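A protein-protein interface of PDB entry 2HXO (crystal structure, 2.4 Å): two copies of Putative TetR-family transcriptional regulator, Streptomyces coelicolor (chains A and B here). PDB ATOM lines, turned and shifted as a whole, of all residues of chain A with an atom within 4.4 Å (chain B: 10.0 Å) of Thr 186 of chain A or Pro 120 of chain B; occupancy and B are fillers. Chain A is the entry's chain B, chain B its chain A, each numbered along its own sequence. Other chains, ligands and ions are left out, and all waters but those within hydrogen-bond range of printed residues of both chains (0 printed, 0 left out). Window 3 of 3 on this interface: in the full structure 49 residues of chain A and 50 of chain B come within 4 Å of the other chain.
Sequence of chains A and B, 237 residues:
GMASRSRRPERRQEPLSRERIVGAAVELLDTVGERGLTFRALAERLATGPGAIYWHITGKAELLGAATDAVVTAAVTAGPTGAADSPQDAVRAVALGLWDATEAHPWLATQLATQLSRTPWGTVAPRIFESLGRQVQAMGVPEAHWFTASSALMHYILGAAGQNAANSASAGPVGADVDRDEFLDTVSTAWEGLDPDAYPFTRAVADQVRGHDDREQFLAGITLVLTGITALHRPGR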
ATOM      1  N   GLU A 182       9.555  15.978  -2.921  1.00  0.00           N
ATOM      2  CA  GLU A 182       9.951  16.853  -1.825  1.00  0.00           C
ATOM      3  C   GLU A 182      10.044  18.292  -2.326  1.00  0.00           C
ATOM      4  O   GLU A 182       9.686  19.234  -1.616  1.00  0.00           O
ATOM      5  CB  GLU A 182      11.284  16.373  -1.238  1.00  0.00           C
ATOM      6  CG  GLU A 182      11.201  14.925  -0.726  1.00  0.00           C
ATOM      7  CD  GLU A 182      12.493  14.403  -0.107  1.00  0.00           C
ATOM      8  OE1 GLU A 182      13.547  14.429  -0.787  1.00  0.00           O
ATOM      9  OE2 GLU A 182      12.446  13.951   1.062  1.00  0.00           O
ATOM     10  N   PHE A 183      10.515  18.457  -3.558  1.00  0.00           N
ATOM     11  CA  PHE A 183      10.620  19.782  -4.164  1.00  0.00           C
ATOM     12  C   PHE A 183       9.209  20.326  -4.384  1.00  0.00           C
ATOM     13  O   PHE A 183       8.934  21.495  -4.134  1.00  0.00           O
ATOM     14  CB  PHE A 183      11.356  19.694  -5.504  1.00  0.00           C
ATOM     15  CG  PHE A 183      11.355  20.978  -6.282  1.00  0.00           C
ATOM     16  CD1 PHE A 183      12.225  22.007  -5.954  1.00  0.00           C
ATOM     17  CD2 PHE A 183      10.470  21.161  -7.337  1.00  0.00           C
ATOM     18  CE1 PHE A 183      12.211  23.202  -6.668  1.00  0.00           C
ATOM     19  CE2 PHE A 183      10.449  22.348  -8.056  1.00  0.00           C
ATOM     20  CZ  PHE A 183      11.320  23.371  -7.720  1.00  0.00           C
ATOM     21  N   LEU A 184       8.310  19.470  -4.850  1.00  0.00           N
ATOM     22  CA  LEU A 184       6.937  19.897  -5.082  1.00  0.00           C
ATOM     23  C   LEU A 184       6.218  20.200  -3.774  1.00  0.00           C
ATOM     24  O   LEU A 184       5.334  21.050  -3.725  1.00  0.00           O
ATOM     25  CB  LEU A 184       6.162  18.825  -5.860  1.00  0.00           C
ATOM     26  CG  LEU A 184       6.629  18.633  -7.303  1.00  0.00           C
ATOM     27  CD1 LEU A 184       5.916  17.449  -7.916  1.00  0.00           C
ATOM     28  CD2 LEU A 184       6.363  19.911  -8.102  1.00  0.00           C
ATOM     29  N   ASP A 185       6.594  19.505  -2.709  1.00  0.00           N
ATOM     30  CA  ASP A 185       5.940  19.749  -1.435  1.00  0.00           C
ATOM     31  C   ASP A 185       6.415  21.057  -0.845  1.00  0.00           C
ATOM     32  O   ASP A 185       5.663  21.730  -0.142  1.00  0.00           O
ATOM     33  CB  ASP A 185       6.202  18.614  -0.445  1.00  0.00           C
ATOM     34  CG  ASP A 185       5.491  18.836   0.886  1.00  0.00           C
ATOM     35  OD1 ASP A 185       6.012  19.611   1.726  1.00  0.00           O
ATOM     36  OD2 ASP A 185       4.400  18.248   1.079  1.00  0.00           O
ATOM     37  N   THR A 186       7.662  21.422  -1.126  1.00  0.00           N
ATOM     38  CA  THR A 186       8.191  22.679  -0.609  1.00  0.00           C
ATOM     39  C   THR A 186       7.602  23.840  -1.430  1.00  0.00           C
ATOM     40  O   THR A 186       7.340  24.923  -0.892  1.00  0.00           O
ATOM     41  CB  THR A 186       9.750  22.692  -0.634  1.00  0.00           C
ATOM     42  OG1 THR A 186      10.224  22.386  -1.950  1.00  0.00           O
ATOM     43  CG2 THR A 186      10.301  21.643   0.312  1.00  0.00           C
ATOM     44  N   VAL A 187       7.369  23.612  -2.724  1.00  0.00           N
ATOM     45  CA  VAL A 187       6.771  24.653  -3.573  1.00  0.00           C
ATOM     46  C   VAL A 187       5.327  24.878  -3.114  1.00  0.00           C
ATOM     47  O   VAL A 187       4.882  26.017  -2.941  1.00  0.00           O
ATOM     48  CB  VAL A 187       6.749  24.266  -5.089  1.00  0.00           C
ATOM     49  CG1 VAL A 187       5.921  25.286  -5.878  1.00  0.00           C
ATOM     50  CG2 VAL A 187       8.156  24.233  -5.655  1.00  0.00           C
ATOM     51  N   SER A 188       4.596  23.784  -2.915  1.00  0.00           N
ATOM     52  CA  SER A 188       3.208  23.880  -2.474  1.00  0.00           C
ATOM     53  C   SER A 188       3.125  24.686  -1.171  1.00  0.00           C
ATOM     54  O   SER A 188       2.262  25.556  -1.007  1.00  0.00           O
ATOM     55  CB  SER A 188       2.635  22.483  -2.260  1.00  0.00           C
ATOM     56  OG  SER A 188       1.265  22.554  -1.939  1.00  0.00           O
ATOM     57  N   THR A 189       4.037  24.389  -0.251  1.00  0.00           N
ATOM     58  CA  THR A 189       4.099  25.076   1.028  1.00  0.00           C
ATOM     59  C   THR A 189       4.378  26.563   0.835  1.00  0.00           C
ATOM     60  O   THR A 189       3.669  27.405   1.377  1.00  0.00           O
ATOM     61  CB  THR A 189       5.190  24.454   1.910  1.00  0.00           C
ATOM     62  OG1 THR A 189       4.844  23.091   2.186  1.00  0.00           O
ATOM     63  CG2 THR A 189       5.333  25.220   3.218  1.00  0.00           C
ATOM     64  N   ALA A 190       5.406  26.885   0.058  1.00  0.00           N
ATOM     65  CA  ALA A 190       5.766  28.278  -0.213  1.00  0.00           C
ATOM     66  C   ALA A 190       4.623  29.069  -0.843  1.00  0.00           C
ATOM     67  O   ALA A 190       4.430  30.247  -0.534  1.00  0.00           O
ATOM     68  CB  ALA A 190       6.994  28.338  -1.126  1.00  0.00           C
ATOM     69  N   ALA B  61      22.883  33.351  -5.800  1.00  0.00           N
ATOM     70  CA  ALA B  61      21.653  32.681  -6.202  1.00  0.00           C
ATOM     71  C   ALA B  61      20.444  33.606  -6.052  1.00  0.00           C
ATOM     72  O   ALA B  61      19.587  33.668  -6.932  1.00  0.00           O
ATOM     73  CB  ALA B  61      21.451  31.411  -5.366  1.00  0.00           C
ATOM     74  N   GLU B  62      20.386  34.322  -4.932  1.00  0.00           N
ATOM     75  CA  GLU B  62      19.292  35.247  -4.652  1.00  0.00           C
ATOM     76  C   GLU B  62      19.343  36.477  -5.568  1.00  0.00           C
ATOM     77  O   GLU B  62      18.304  37.033  -5.939  1.00  0.00           O
ATOM     78  CB  GLU B  62      19.339  35.701  -3.188  1.00  0.00           C
ATOM     79  CG  GLU B  62      19.036  34.631  -2.124  1.00  0.00           C
ATOM     80  CD  GLU B  62      19.931  33.389  -2.201  1.00  0.00           C
ATOM     81  OE1 GLU B  62      21.175  33.527  -2.333  1.00  0.00           O
ATOM     82  OE2 GLU B  62      19.377  32.262  -2.118  1.00  0.00           O
ATOM     83  N   LEU B 112      15.373  30.927 -15.766  1.00  0.00           N
ATOM     84  CA  LEU B 112      13.995  30.479 -15.598  1.00  0.00           C
ATOM     85  C   LEU B 112      13.941  28.969 -15.358  1.00  0.00           C
ATOM     86  O   LEU B 112      13.143  28.483 -14.553  1.00  0.00           O
ATOM     87  CB  LEU B 112      13.168  30.841 -16.829  1.00  0.00           C
ATOM     88  CG  LEU B 112      12.898  32.327 -17.073  1.00  0.00           C
ATOM     89  CD1 LEU B 112      12.233  32.496 -18.430  1.00  0.00           C
ATOM     90  CD2 LEU B 112      12.014  32.891 -15.968  1.00  0.00           C
ATOM     91  N   ALA B 113      14.798  28.225 -16.050  1.00  0.00           N
ATOM     92  CA  ALA B 113      14.842  26.776 -15.880  1.00  0.00           C
ATOM     93  C   ALA B 113      15.304  26.432 -14.466  1.00  0.00           C
ATOM     94  O   ALA B 113      14.767  25.531 -13.824  1.00  0.00           O
ATOM     95  CB  ALA B 113      15.789  26.155 -16.901  1.00  0.00           C
ATOM     96  N   THR B 114      16.312  27.153 -13.990  1.00  0.00           N
ATOM     97  CA  THR B 114      16.844  26.935 -12.652  1.00  0.00           C
ATOM     98  C   THR B 114      15.837  27.414 -11.620  1.00  0.00           C
ATOM     99  O   THR B 114      15.732  26.855 -10.532  1.00  0.00           O
ATOM    100  CB  THR B 114      18.174  27.689 -12.455  1.00  0.00           C
ATOM    101  OG1 THR B 114      18.005  29.062 -12.816  1.00  0.00           O
ATOM    102  CG2 THR B 114      19.262  27.071 -13.321  1.00  0.00           C
ATOM    103  N   GLN B 115      15.085  28.444 -11.985  1.00  0.00           N
ATOM    104  CA  GLN B 115      14.079  29.016 -11.108  1.00  0.00           C
ATOM    105  C   GLN B 115      12.957  28.014 -10.856  1.00  0.00           C
ATOM    106  O   GLN B 115      12.431  27.930  -9.748  1.00  0.00           O
ATOM    107  CB  GLN B 115      13.507  30.281 -11.743  1.00  0.00           C
ATOM    108  CG  GLN B 115      12.846  31.229 -10.775  1.00  0.00           C
ATOM    109  CD  GLN B 115      13.839  31.990  -9.919  1.00  0.00           C
ATOM    110  OE1 GLN B 115      13.560  32.079  -8.625  1.00  0.00           O
ATOM    111  NE2 GLN B 115      14.839  32.505 -10.418  1.00  0.00           N
ATOM    112  N   LEU B 116      12.602  27.246 -11.884  1.00  0.00           N
ATOM    113  CA  LEU B 116      11.527  26.264 -11.765  1.00  0.00           C
ATOM    114  C   LEU B 116      12.015  24.872 -11.380  1.00  0.00           C
ATOM    115  O   LEU B 116      11.211  23.957 -11.199  1.00  0.00           O
ATOM    116  CB  LEU B 116      10.753  26.160 -13.079  1.00  0.00           C
ATOM    117  CG  LEU B 116      10.432  27.456 -13.822  1.00  0.00           C
ATOM    118  CD1 LEU B 116       9.533  27.139 -14.997  1.00  0.00           C
ATOM    119  CD2 LEU B 116       9.771  28.451 -12.896  1.00  0.00           C
ATOM    120  N   SER B 117      13.323  24.706 -11.243  1.00  0.00           N
ATOM    121  CA  SER B 117      13.875  23.403 -10.898  1.00  0.00           C
ATOM    122  C   SER B 117      14.489  23.313  -9.506  1.00  0.00           C
ATOM    123  O   SER B 117      14.412  22.264  -8.860  1.00  0.00           O
ATOM    124  CB  SER B 117      14.931  23.003 -11.927  1.00  0.00           C
ATOM    125  OG  SER B 117      14.370  22.949 -13.226  1.00  0.00           O
ATOM    126  N   ARG B 118      15.100  24.400  -9.040  1.00  0.00           N
ATOM    127  CA  ARG B 118      15.751  24.372  -7.735  1.00  0.00           C
ATOM    128  C   ARG B 118      15.421  25.545  -6.831  1.00  0.00           C
ATOM    129  O   ARG B 118      16.001  25.669  -5.750  1.00  0.00           O
ATOM    130  CB  ARG B 118      17.273  24.315  -7.913  1.00  0.00           C
ATOM    131  CG  ARG B 118      17.751  23.517  -9.123  1.00  0.00           C
ATOM    132  CD  ARG B 118      19.247  23.225  -9.026  1.00  0.00           C
ATOM    133  NE  ARG B 118      20.006  24.399  -8.600  1.00  0.00           N
ATOM    134  CZ  ARG B 118      20.104  25.524  -9.301  1.00  0.00           C
ATOM    135  NH1 ARG B 118      19.495  25.633 -10.475  1.00  0.00           N
ATOM    136  NH2 ARG B 118      20.805  26.546  -8.821  1.00  0.00           N
ATOM    137  N   THR B 119      14.499  26.404  -7.256  1.00  0.00           N
ATOM    138  CA  THR B 119      14.145  27.573  -6.457  1.00  0.00           C
ATOM    139  C   THR B 119      12.707  27.540  -5.955  1.00  0.00           C
ATOM    140  O   THR B 119      11.862  28.309  -6.417  1.00  0.00           O
ATOM    141  CB  THR B 119      14.345  28.860  -7.262  1.00  0.00           C
ATOM    142  OG1 THR B 119      15.592  28.791  -7.958  1.00  0.00           O
ATOM    143  CG2 THR B 119      14.353  30.068  -6.339  1.00  0.00           C
ATOM    144  N   PRO B 120      12.417  26.661  -4.982  1.00  0.00           N
ATOM    145  CA  PRO B 120      11.076  26.520  -4.405  1.00  0.00           C
ATOM    146  C   PRO B 120      10.452  27.839  -3.943  1.00  0.00           C
ATOM    147  O   PRO B 120       9.249  28.054  -4.093  1.00  0.00           O
ATOM    148  CB  PRO B 120      11.307  25.561  -3.236  1.00  0.00           C
ATOM    149  CG  PRO B 120      12.445  24.717  -3.712  1.00  0.00           C
ATOM    150  CD  PRO B 120      13.365  25.738  -4.333  1.00  0.00           C
ATOM    151  N   TRP B 121      11.272  28.718  -3.381  1.00  0.00           N
ATOM    152  CA  TRP B 121      10.779  29.994  -2.888  1.00  0.00           C
ATOM    153  C   TRP B 121      10.897  31.138  -3.884  1.00  0.00           C
ATOM    154  O   TRP B 121      10.680  32.297  -3.531  1.00  0.00           O
ATOM    155  CB  TRP B 121      11.490  30.343  -1.575  1.00  0.00           C
ATOM    156  CG  TRP B 121      10.830  29.687  -0.385  1.00  0.00           C
ATOM    157  CD1 TRP B 121       9.658  30.069   0.219  1.00  0.00           C
ATOM    158  CD2 TRP B 121      11.255  28.495   0.286  1.00  0.00           C
ATOM    159  NE1 TRP B 121       9.330  29.184   1.219  1.00  0.00           N
ATOM    160  CE2 TRP B 121      10.291  28.208   1.282  1.00  0.00           C
ATOM    161  CE3 TRP B 121      12.355  27.638   0.143  1.00  0.00           C
ATOM    162  CZ2 TRP B 121      10.394  27.100   2.130  1.00  0.00           C
ATOM    163  CZ3 TRP B 121      12.459  26.534   0.987  1.00  0.00           C
ATOM    164  CH2 TRP B 121      11.482  26.277   1.969  1.00  0.00           C
ATOM    165  N   GLY B 122      11.229  30.805  -5.128  1.00  0.00           N
ATOM    166  CA  GLY B 122      11.370  31.820  -6.156  1.00  0.00           C
ATOM    167  C   GLY B 122      10.104  32.636  -6.338  1.00  0.00           C
ATOM    168  O   GLY B 122       8.996  32.133  -6.173  1.00  0.00           O
ATOM    169  N   THR B 123      10.264  33.900  -6.699  1.00  0.00           N
ATOM    170  CA  THR B 123       9.120  34.773  -6.878  1.00  0.00           C
ATOM    171  C   THR B 123       8.655  34.911  -8.322  1.00  0.00           C
ATOM    172  O   THR B 123       7.540  35.353  -8.568  1.00  0.00           O
ATOM    173  CB  THR B 123       9.426  36.173  -6.362  1.00  0.00           C
ATOM    174  OG1 THR B 123      10.412  36.773  -7.207  1.00  0.00           O
ATOM    175  CG2 THR B 123       9.956  36.105  -4.935  1.00  0.00           C
ATOM    176  N   VAL B 124       9.497  34.541  -9.279  1.00  0.00           N
ATOM    177  CA  VAL B 124       9.102  34.696 -10.665  1.00  0.00           C
ATOM    178  C   VAL B 124       8.066  33.658 -11.090  1.00  0.00           C
ATOM    179  O   VAL B 124       7.087  33.993 -11.755  1.00  0.00           O
ATOM    180  CB  VAL B 124      10.316  34.629 -11.623  1.00  0.00           C
ATOM    181  CG1 VAL B 124      10.837  33.231 -11.706  1.00  0.00           C
ATOM    182  CG2 VAL B 124       9.907  35.108 -13.018  1.00  0.00           C
ATOM    183  N   ALA B 125       8.272  32.409 -10.684  1.00  0.00           N
ATOM    184  CA  ALA B 125       7.360  31.337 -11.047  1.00  0.00           C
ATOM    185  C   ALA B 125       5.913  31.645 -10.663  1.00  0.00           C
ATOM    186  O   ALA B 125       5.037  31.698 -11.528  1.00  0.00           O
ATOM    187  CB  ALA B 125       7.807  30.032 -10.415  1.00  0.00           C
ATOM    188  N   PRO B 126       5.640  31.860  -9.362  1.00  0.00           N
ATOM    189  CA  PRO B 126       4.266  32.158  -8.936  1.00  0.00           C
ATOM    190  C   PRO B 126       3.638  33.378  -9.610  1.00  0.00           C
ATOM    191  O   PRO B 126       2.429  33.427  -9.806  1.00  0.00           O
ATOM    192  CB  PRO B 126       4.397  32.310  -7.413  1.00  0.00           C
ATOM    193  CG  PRO B 126       5.824  32.718  -7.228  1.00  0.00           C
ATOM    194  CD  PRO B 126       6.550  31.844  -8.204  1.00  0.00           C
ATOM    195  N   ARG B 127       4.449  34.362  -9.968  1.00  0.00           N
ATOM    196  CA  ARG B 127       3.906  35.545 -10.633  1.00  0.00           C
ATOM    197  C   ARG B 127       3.479  35.247 -12.085  1.00  0.00           C
ATOM    198  O   ARG B 127       2.471  35.766 -12.560  1.00  0.00           O
ATOM    199  CB  ARG B 127       4.924  36.686 -10.569  1.00  0.00           C
ATOM    200  CG  ARG B 127       5.002  37.269  -9.171  1.00  0.00           C
ATOM    201  CD  ARG B 127       6.169  38.210  -8.960  1.00  0.00           C
ATOM    202  NE  ARG B 127       6.017  38.909  -7.689  1.00  0.00           N
ATOM    203  CZ  ARG B 127       7.009  39.479  -7.008  1.00  0.00           C
ATOM    204  NH1 ARG B 127       8.251  39.441  -7.473  1.00  0.00           N
ATOM    205  NH2 ARG B 127       6.756  40.072  -5.847  1.00  0.00           N
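The backbone carbonyl oxygen of Ala 113 of chain B is in hydrogen-bond range of the side-chain hydroxyl of Ser 117 of chain B, at 2.7 Å. The backbone carbonyl oxygen (O) of Thr 114 of chain B lies within hydrogen-bond range of the side-chain hydroxyl (OG1) of Thr 119 of chain B. O of Glu 182 of chain A lies close to OG1 of Thr 186 of chain A (3.2 Å). The backbone carbonyl oxygen (O) of Phe 183 of chain A is in hydrogen-bond range of the side-chain hydroxyl (OG1) of Thr 186 of chain A, at 2.7 Å.
Leu 116 of chain B touches Phe 183 of chain A. Ser 117 of chain B touches Phe 183 of chain A. Phe 183 of chain A touches Arg 118 of chain B. Phe 183 of chain A touches Thr 119 of chain B (CE1 to N, 3.98 Å). Phe 183 of chain A touches Pro 120 of chain B. CB of Pro 120 of chain B touches OG1 of Thr 186 of chain A, 3.6 Å away. Val 187 of chain A touches Pro 120 of chain B (CG2 to CA, 3.9 Å). O of Pro 120 of chain B touches CB of Ala 190 of chain A, 3.7 Å away. Trp 121 of chain B touches Ala 190 of chain A.
Thr 186 of chain A touches just one residue of chain B: Pro 120. Of chain A, only Phe 183, Thr 186, Val 187 and Ala 190 come within 4 Å of Pro 120 of chain B. Phe 183 of chain A touches five residues of chain B. No residue of chain B comes within 4 Å of Asp 185 of chain A. Printed residues of chain B within 4 Å of Val 187 of chain A: Pro 120 (3.9 Å). No residue of chain B comes within 4 Å of Thr 189 of chain A. Of the printed residues of chain A, Trp 121 of chain B touches Ala 190. Printed residues of chain B within 4 Å of Ala 190 of chain A: Pro 120 and Trp 121. Of the printed residues of chain A, Arg 118 of chain B touches Phe 183 (3.9 Å). Of the printed residues of chain A, Thr 119 of chain B touches Phe 183 (3.98 Å). Of the printed residues of chain A, Ser 117 of chain B touches Phe 183 (3.2 Å). Val 124 of chain B touches none of the printed residues of chain A. Pro 126 of chain B touches none of the printed residues of chain A.
Hydrophobic or aromatic side chains of chain B that line the printed part of chain A: Pro 120 and Trp 121. Of the 9 printed residues of chain A, 4 touch a printed residue of chain B. Printed residues of chain A that touch a printed residue of chain B: Phe 183, Thr 186, Val 187 and Ala 190.
No position is printed for both chains. Of the 9 pairs that touch across the chains among the printed residues, none has its exchanged pair printed and touching as well.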
